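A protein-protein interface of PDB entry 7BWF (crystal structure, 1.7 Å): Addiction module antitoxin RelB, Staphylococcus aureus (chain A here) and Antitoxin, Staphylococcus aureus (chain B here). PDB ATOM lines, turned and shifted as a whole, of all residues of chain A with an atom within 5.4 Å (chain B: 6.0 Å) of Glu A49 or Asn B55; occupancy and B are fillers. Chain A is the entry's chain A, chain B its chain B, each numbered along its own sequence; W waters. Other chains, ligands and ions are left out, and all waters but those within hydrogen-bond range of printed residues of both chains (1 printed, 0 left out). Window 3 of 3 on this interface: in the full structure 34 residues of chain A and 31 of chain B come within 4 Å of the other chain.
Among the printed residues, merely in contact across the chains: Leu A51 with Thr B60 (3.8 Å) and Glu A49 with Ser B52 (3.9 Å).
Of the 11 printed residues of chain B, 5 touch a printed residue of chain A. Printed residues of chain B that touch a printed residue of chain A: Ser B52, Asn B55, Ser B56, Glu B59 and Thr B60. Of the 10 printed residues of chain A, 4 touch a printed residue of chain B. Printed residues of chain A that touch a printed residue of chain B: Glu A49, Lys A50, Leu A51 and Ser A60. Along chain A the printed residues that touch a printed residue of chain B span positions 49 to 60. Among the printed residues, 5 pairs touch across the chains. Among the printed residues, no Asp or Glu carboxylate lies within 4 Å of a Lys or Arg side-chain nitrogen of the other chain.
Water W1 lies within hydrogen-bond range of the side-chain hydroxyl of Ser B56 (2.5 Å), the side-chain carboxylate of Glu A49 (2.6 Å), the backbone NH of Lys A50 (3.1 Å) and the backbone carbonyl oxygen of Ser B52 (3.4 Å).
Of chain B, only Ser B52 and Asn B55 come within 4 Å of Glu A49. Asn B55 touches one residue of chain A. Printed residues of chain A within 4 Å of Glu B59: Ser A60 (2.7 Å). Printed residues of chain A within 4 Å of Ser B52: Glu A49 (3.9 Å). Met B57 touches none of the printed residues of chain A. Ser B50 touches none of the printed residues of chain A. The nearest printed residue of chain B that does not touch Glu A49 is Ser B56 (4.2 Å). The nearest printed residue of chain B that does not touch Lys A50 is Thr B60 (4.8 Å).
O of Glu A49 lies within hydrogen-bond range of N of Ser A60 (3.0 Å). The backbone NH (N) of Leu A51 sits at hydrogen-bond distance from the backbone carbonyl oxygen (O) of Tyr A58 (3.0 Å). The side-chain amide nitrogen (ND2) of Asn B55 lies close to the backbone carbonyl oxygen (O) of Glu B51, at 3.5 Å. The backbone carbonyl oxygen (O) of Ser B52 sits at hydrogen-bond distance from the side-chain hydroxyl (OG) of Ser B56 (3.1 Å). OG1 of Thr B60 sits at hydrogen-bond distance from O of Ser B56 (2.8 Å).
The side-chain carboxylate (OE2) of Glu A49 is in hydrogen-bond range of the side-chain amide nitrogen (ND2) of Asn B55 (3.2 Å). The backbone carbonyl oxygen (O) of Lys A50 is in hydrogen-bond range of the side-chain hydroxyl (OG) of Ser B56 (2.7 Å). The side-chain carboxylate (OE2) of Glu B59 lies within hydrogen-bond range of the side-chain hydroxyl (OG) of Ser A60 (2.7 Å).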
ATOM      1  N   LEU A  42     -19.591 -28.559 -14.257  1.00  0.00           N
ATOM      2  CA  LEU A  42     -20.988 -28.570 -13.829  1.00  0.00           C
ATOM      3  C   LEU A  42     -21.170 -28.806 -12.334  1.00  0.00           C
ATOM      4  O   LEU A  42     -22.296 -29.066 -11.889  1.00  0.00           O
ATOM      5  CB  LEU A  42     -21.769 -29.635 -14.610  1.00  0.00           C
ATOM      6  CG  LEU A  42     -22.272 -29.217 -15.996  1.00  0.00           C
ATOM      7  CD1 LEU A  42     -23.019 -30.354 -16.694  1.00  0.00           C
ATOM      8  CD2 LEU A  42     -23.159 -27.974 -15.907  1.00  0.00           C
ATOM      9  N   LYS A  47     -23.848 -22.109  -8.938  1.00  0.00           N
ATOM     10  CA  LYS A  47     -24.993 -22.639  -9.644  1.00  0.00           C
ATOM     11  C   LYS A  47     -24.643 -22.891 -11.128  1.00  0.00           C
ATOM     12  O   LYS A  47     -25.190 -22.210 -12.004  1.00  0.00           O
ATOM     13  CB  LYS A  47     -26.187 -21.712  -9.546  1.00  0.00           C
ATOM     14  CG  LYS A  47     -26.470 -21.283  -8.169  1.00  0.00           C
ATOM     15  CD  LYS A  47     -27.790 -20.564  -8.068  1.00  0.00           C
ATOM     16  CE  LYS A  47     -28.751 -21.261  -7.102  1.00  0.00           C
ATOM     17  NZ  LYS A  47     -28.313 -21.211  -5.677  1.00  0.00           N
ATOM     18  N   PRO A  48     -23.713 -23.783 -11.407  1.00  0.00           N
ATOM     19  CA  PRO A  48     -23.319 -24.016 -12.804  1.00  0.00           C
ATOM     20  C   PRO A  48     -24.506 -24.453 -13.637  1.00  0.00           C
ATOM     21  O   PRO A  48     -25.329 -25.255 -13.190  1.00  0.00           O
ATOM     22  CB  PRO A  48     -22.271 -25.129 -12.716  1.00  0.00           C
ATOM     23  CG  PRO A  48     -22.056 -25.444 -11.288  1.00  0.00           C
ATOM     24  CD  PRO A  48     -22.893 -24.530 -10.444  1.00  0.00           C
ATOM     25  N   GLU A  49     -24.607 -23.890 -14.844  1.00  0.00           N
ATOM     26  CA  GLU A  49     -25.625 -24.295 -15.799  1.00  0.00           C
ATOM     27  C   GLU A  49     -25.050 -24.365 -17.207  1.00  0.00           C
ATOM     28  O   GLU A  49     -24.216 -23.543 -17.596  1.00  0.00           O
ATOM     29  CB  GLU A  49     -26.806 -23.311 -15.798  1.00  0.00           C
ATOM     30  CG  GLU A  49     -27.457 -23.099 -14.428  1.00  0.00           C
ATOM     31  CD  GLU A  49     -28.282 -24.292 -13.971  1.00  0.00           C
ATOM     32  OE1 GLU A  49     -28.405 -25.256 -14.754  1.00  0.00           O
ATOM     33  OE2 GLU A  49     -28.817 -24.261 -12.840  1.00  0.00           O
ATOM     34  N   LYS A  50     -25.521 -25.346 -17.968  1.00  0.00           N
ATOM     35  CA  LYS A  50     -25.250 -25.430 -19.393  1.00  0.00           C
ATOM     36  C   LYS A  50     -26.018 -24.338 -20.128  1.00  0.00           C
ATOM     37  O   LYS A  50     -27.190 -24.077 -19.835  1.00  0.00           O
ATOM     38  CB  LYS A  50     -25.676 -26.802 -19.924  1.00  0.00           C
ATOM     39  CG  LYS A  50     -24.724 -27.955 -19.684  1.00  0.00           C
ATOM     40  CD  LYS A  50     -25.270 -29.188 -20.415  1.00  0.00           C
ATOM     41  CE  LYS A  50     -24.428 -29.554 -21.620  1.00  0.00           C
ATOM     42  NZ  LYS A  50     -23.043 -29.843 -21.180  1.00  0.00           N
ATOM     43  N   LEU A  51     -25.362 -23.717 -21.100  1.00  0.00           N
ATOM     44  CA  LEU A  51     -25.991 -22.718 -21.951  1.00  0.00           C
ATOM     45  C   LEU A  51     -26.419 -23.351 -23.268  1.00  0.00           C
ATOM     46  O   LEU A  51     -25.870 -24.363 -23.712  1.00  0.00           O
ATOM     47  CB  LEU A  51     -25.047 -21.539 -22.220  1.00  0.00           C
ATOM     48  CG  LEU A  51     -24.619 -20.842 -20.925  1.00  0.00           C
ATOM     49  CD1 LEU A  51     -23.695 -19.649 -21.186  1.00  0.00           C
ATOM     50  CD2 LEU A  51     -25.821 -20.387 -20.071  1.00  0.00           C
ATOM     51  N   TYR A  58     -20.918 -23.793 -23.759  1.00  0.00           N
ATOM     52  CA  TYR A  58     -20.437 -22.983 -22.658  1.00  0.00           C
ATOM     53  C   TYR A  58     -21.328 -23.143 -21.439  1.00  0.00           C
ATOM     54  O   TYR A  58     -22.413 -23.721 -21.487  1.00  0.00           O
ATOM     55  CB  TYR A  58     -20.347 -21.516 -23.075  1.00  0.00           C
ATOM     56  CG  TYR A  58     -19.128 -21.249 -23.922  1.00  0.00           C
ATOM     57  CD1 TYR A  58     -19.082 -21.656 -25.248  1.00  0.00           C
ATOM     58  CD2 TYR A  58     -18.016 -20.608 -23.395  1.00  0.00           C
ATOM     59  CE1 TYR A  58     -17.965 -21.425 -26.025  1.00  0.00           C
ATOM     60  CE2 TYR A  58     -16.896 -20.370 -24.169  1.00  0.00           C
ATOM     61  CZ  TYR A  58     -16.875 -20.783 -25.481  1.00  0.00           C
ATOM     62  OH  TYR A  58     -15.757 -20.545 -26.246  1.00  0.00           O
ATOM     63  N   TYR A  59     -20.825 -22.630 -20.325  1.00  0.00           N
ATOM     64  CA  TYR A  59     -21.491 -22.725 -19.038  1.00  0.00           C
ATOM     65  C   TYR A  59     -21.497 -21.344 -18.404  1.00  0.00           C
ATOM     66  O   TYR A  59     -20.704 -20.473 -18.765  1.00  0.00           O
ATOM     67  CB  TYR A  59     -20.786 -23.717 -18.094  1.00  0.00           C
ATOM     68  CG  TYR A  59     -20.522 -25.064 -18.723  1.00  0.00           C
ATOM     69  CD1 TYR A  59     -19.414 -25.261 -19.531  1.00  0.00           C
ATOM     70  CD2 TYR A  59     -21.365 -26.140 -18.495  1.00  0.00           C
ATOM     71  CE1 TYR A  59     -19.160 -26.491 -20.109  1.00  0.00           C
ATOM     72  CE2 TYR A  59     -21.117 -27.375 -19.067  1.00  0.00           C
ATOM     73  CZ  TYR A  59     -20.017 -27.545 -19.870  1.00  0.00           C
ATOM     74  OH  TYR A  59     -19.775 -28.778 -20.436  1.00  0.00           O
ATOM     75  N   SER A  60     -22.378 -21.161 -17.426  1.00  0.00           N
ATOM     76  CA  SER A  60     -22.389 -19.937 -16.639  1.00  0.00           C
ATOM     77  C   SER A  60     -22.421 -20.267 -15.157  1.00  0.00           C
ATOM     78  O   SER A  60     -23.086 -21.216 -14.725  1.00  0.00           O
ATOM     79  CB  SER A  60     -23.588 -19.036 -16.993  1.00  0.00           C
ATOM     80  OG  SER A  60     -24.747 -19.380 -16.249  1.00  0.00           O
ATOM     81  N   ARG A  61     -21.674 -19.481 -14.396  1.00  0.00           N
ATOM     82  CA  ARG A  61     -21.726 -19.477 -12.947  1.00  0.00           C
ATOM     83  C   ARG A  61     -21.976 -18.048 -12.497  1.00  0.00           C
ATOM     84  O   ARG A  61     -21.609 -17.090 -13.183  1.00  0.00           O
ATOM     85  CB  ARG A  61     -20.429 -20.014 -12.340  1.00  0.00           C
ATOM     86  CG  ARG A  61     -20.375 -21.534 -12.299  1.00  0.00           C
ATOM     87  CD  ARG A  61     -19.134 -22.055 -11.600  1.00  0.00           C
ATOM     88  NE  ARG A  61     -18.791 -23.410 -12.030  1.00  0.00           N
ATOM     89  CZ  ARG A  61     -18.391 -24.385 -11.213  1.00  0.00           C
ATOM     90  NH1 ARG A  61     -18.280 -24.174  -9.905  1.00  0.00           N
ATOM     91  NH2 ARG A  61     -18.097 -25.580 -11.707  1.00  0.00           N
ATOM     92  N   SER B  50     -36.914 -30.820 -17.484  1.00  0.00           N
ATOM     93  CA  SER B  50     -36.039 -30.964 -16.332  1.00  0.00           C
ATOM     94  C   SER B  50     -35.759 -29.589 -15.741  1.00  0.00           C
ATOM     95  O   SER B  50     -35.732 -28.582 -16.451  1.00  0.00           O
ATOM     96  CB  SER B  50     -34.725 -31.650 -16.727  1.00  0.00           C
ATOM     97  OG  SER B  50     -33.916 -30.824 -17.547  1.00  0.00           O
ATOM     98  N   GLU B  51     -35.591 -29.543 -14.419  1.00  0.00           N
ATOM     99  CA  GLU B  51     -35.225 -28.290 -13.768  1.00  0.00           C
ATOM    100  C   GLU B  51     -33.947 -27.726 -14.381  1.00  0.00           C
ATOM    101  O   GLU B  51     -33.804 -26.507 -14.535  1.00  0.00           O
ATOM    102  CB  GLU B  51     -35.048 -28.502 -12.259  1.00  0.00           C
ATOM    103  CG  GLU B  51     -34.752 -27.218 -11.492  1.00  0.00           C
ATOM    104  CD  GLU B  51     -34.652 -27.456  -9.990  1.00  0.00           C
ATOM    105  OE1 GLU B  51     -34.293 -28.582  -9.593  1.00  0.00           O
ATOM    106  OE2 GLU B  51     -34.922 -26.525  -9.212  1.00  0.00           O
ATOM    107  N   SER B  52     -33.011 -28.606 -14.750  1.00  0.00           N
ATOM    108  CA  SER B  52     -31.747 -28.160 -15.329  1.00  0.00           C
ATOM    109  C   SER B  52     -31.982 -27.462 -16.660  1.00  0.00           C
ATOM    110  O   SER B  52     -31.473 -26.364 -16.891  1.00  0.00           O
ATOM    111  CB  SER B  52     -30.782 -29.342 -15.507  1.00  0.00           C
ATOM    112  OG  SER B  52     -30.303 -29.813 -14.262  1.00  0.00           O
ATOM    113  N   ASP B  53     -32.748 -28.088 -17.557  1.00  0.00           N
ATOM    114  CA  ASP B  53     -33.072 -27.440 -18.827  1.00  0.00           C
ATOM    115  C   ASP B  53     -33.831 -26.145 -18.599  1.00  0.00           C
ATOM    116  O   ASP B  53     -33.611 -25.157 -19.306  1.00  0.00           O
ATOM    117  CB  ASP B  53     -33.879 -28.381 -19.716  1.00  0.00           C
ATOM    118  CG  ASP B  53     -33.014 -29.446 -20.353  1.00  0.00           C
ATOM    119  OD1 ASP B  53     -31.772 -29.313 -20.300  1.00  0.00           O
ATOM    120  OD2 ASP B  53     -33.565 -30.425 -20.881  1.00  0.00           O
ATOM    121  N   TYR B  54     -34.696 -26.108 -17.590  1.00  0.00           N
ATOM    122  CA  TYR B  54     -35.368 -24.856 -17.281  1.00  0.00           C
ATOM    123  C   TYR B  54     -34.356 -23.773 -16.936  1.00  0.00           C
ATOM    124  O   TYR B  54     -34.386 -22.675 -17.497  1.00  0.00           O
ATOM    125  CB  TYR B  54     -36.328 -25.017 -16.117  1.00  0.00           C
ATOM    126  CG  TYR B  54     -36.885 -23.680 -15.688  1.00  0.00           C
ATOM    127  CD1 TYR B  54     -37.735 -22.978 -16.517  1.00  0.00           C
ATOM    128  CD2 TYR B  54     -36.512 -23.093 -14.486  1.00  0.00           C
ATOM    129  CE1 TYR B  54     -38.241 -21.757 -16.153  1.00  0.00           C
ATOM    130  CE2 TYR B  54     -37.026 -21.857 -14.101  1.00  0.00           C
ATOM    131  CZ  TYR B  54     -37.905 -21.201 -14.944  1.00  0.00           C
ATOM    132  OH  TYR B  54     -38.446 -19.971 -14.628  1.00  0.00           O
ATOM    133  N   ASN B  55     -33.467 -24.062 -15.984  1.00  0.00           N
ATOM    134  CA  ASN B  55     -32.466 -23.083 -15.580  1.00  0.00           C
ATOM    135  C   ASN B  55     -31.581 -22.700 -16.760  1.00  0.00           C
ATOM    136  O   ASN B  55     -31.202 -21.534 -16.903  1.00  0.00           O
ATOM    137  CB  ASN B  55     -31.617 -23.635 -14.428  1.00  0.00           C
ATOM    138  CG  ASN B  55     -32.389 -23.751 -13.126  1.00  0.00           C
ATOM    139  OD1 ASN B  55     -33.387 -23.059 -12.918  1.00  0.00           O
ATOM    140  ND2 ASN B  55     -31.955 -24.661 -12.261  1.00  0.00           N
ATOM    141  N   SER B  56     -31.252 -23.666 -17.625  1.00  0.00           N
ATOM    142  CA  SER B  56     -30.446 -23.371 -18.808  1.00  0.00           C
ATOM    143  C   SER B  56     -31.156 -22.363 -19.710  1.00  0.00           C
ATOM    144  O   SER B  56     -30.549 -21.394 -20.178  1.00  0.00           O
ATOM    145  CB  SER B  56     -30.134 -24.668 -19.575  1.00  0.00           C
ATOM    146  OG  SER B  56     -29.234 -25.497 -18.854  1.00  0.00           O
ATOM    147  N   MET B  57     -32.455 -22.569 -19.948  1.00  0.00           N
ATOM    148  CA  MET B  57     -33.209 -21.668 -20.817  1.00  0.00           C
ATOM    149  C   MET B  57     -33.247 -20.253 -20.244  1.00  0.00           C
ATOM    150  O   MET B  57     -33.022 -19.279 -20.967  1.00  0.00           O
ATOM    151  CB  MET B  57     -34.633 -22.198 -21.031  1.00  0.00           C
ATOM    152  CG  MET B  57     -34.704 -23.519 -21.771  1.00  0.00           C
ATOM    153  SD  MET B  57     -36.392 -24.095 -22.053  1.00  0.00           S
ATOM    154  CE  MET B  57     -37.323 -22.565 -22.195  1.00  0.00           C
ATOM    155  N   MET B  58     -33.520 -20.122 -18.942  1.00  0.00           N
ATOM    156  CA  MET B  58     -33.616 -18.802 -18.319  1.00  0.00           C
ATOM    157  C   MET B  58     -32.248 -18.132 -18.235  1.00  0.00           C
ATOM    158  O   MET B  58     -32.138 -16.914 -18.411  1.00  0.00           O
ATOM    159  CB  MET B  58     -34.256 -18.927 -16.929  1.00  0.00           C
ATOM    160  CG  MET B  58     -35.569 -19.713 -16.929  1.00  0.00           C
ATOM    161  SD  MET B  58     -36.781 -19.136 -18.145  1.00  0.00           S
ATOM    162  CE  MET B  58     -37.090 -17.454 -17.639  1.00  0.00           C
ATOM    163  N   GLU B  59     -31.191 -18.912 -17.979  1.00  0.00           N
ATOM    164  CA  GLU B  59     -29.835 -18.365 -17.992  1.00  0.00           C
ATOM    165  C   GLU B  59     -29.453 -17.893 -19.393  1.00  0.00           C
ATOM    166  O   GLU B  59     -28.878 -16.813 -19.555  1.00  0.00           O
ATOM    167  CB  GLU B  59     -28.829 -19.412 -17.486  1.00  0.00           C
ATOM    168  CG  GLU B  59     -28.576 -19.368 -15.990  1.00  0.00           C
ATOM    169  CD  GLU B  59     -27.989 -18.037 -15.532  1.00  0.00           C
ATOM    170  OE1 GLU B  59     -28.672 -17.327 -14.780  1.00  0.00           O
ATOM    171  OE2 GLU B  59     -26.853 -17.701 -15.922  1.00  0.00           O
ATOM    172  N   THR B  60     -29.774 -18.684 -20.417  1.00  0.00           N
ATOM    173  CA  THR B  60     -29.510 -18.283 -21.796  1.00  0.00           C
ATOM    174  C   THR B  60     -30.278 -17.017 -22.149  1.00  0.00           C
ATOM    175  O   THR B  60     -29.727 -16.081 -22.737  1.00  0.00           O
ATOM    176  CB  THR B  60     -29.893 -19.420 -22.742  1.00  0.00           C
ATOM    177  OG1 THR B  60     -29.108 -20.575 -22.428  1.00  0.00           O
ATOM    178  CG2 THR B  60     -29.627 -19.018 -24.182  1.00  0.00           C
HETATM  179  O   HOH W   1     -28.109 -26.610 -16.940  1.00  0.00           O
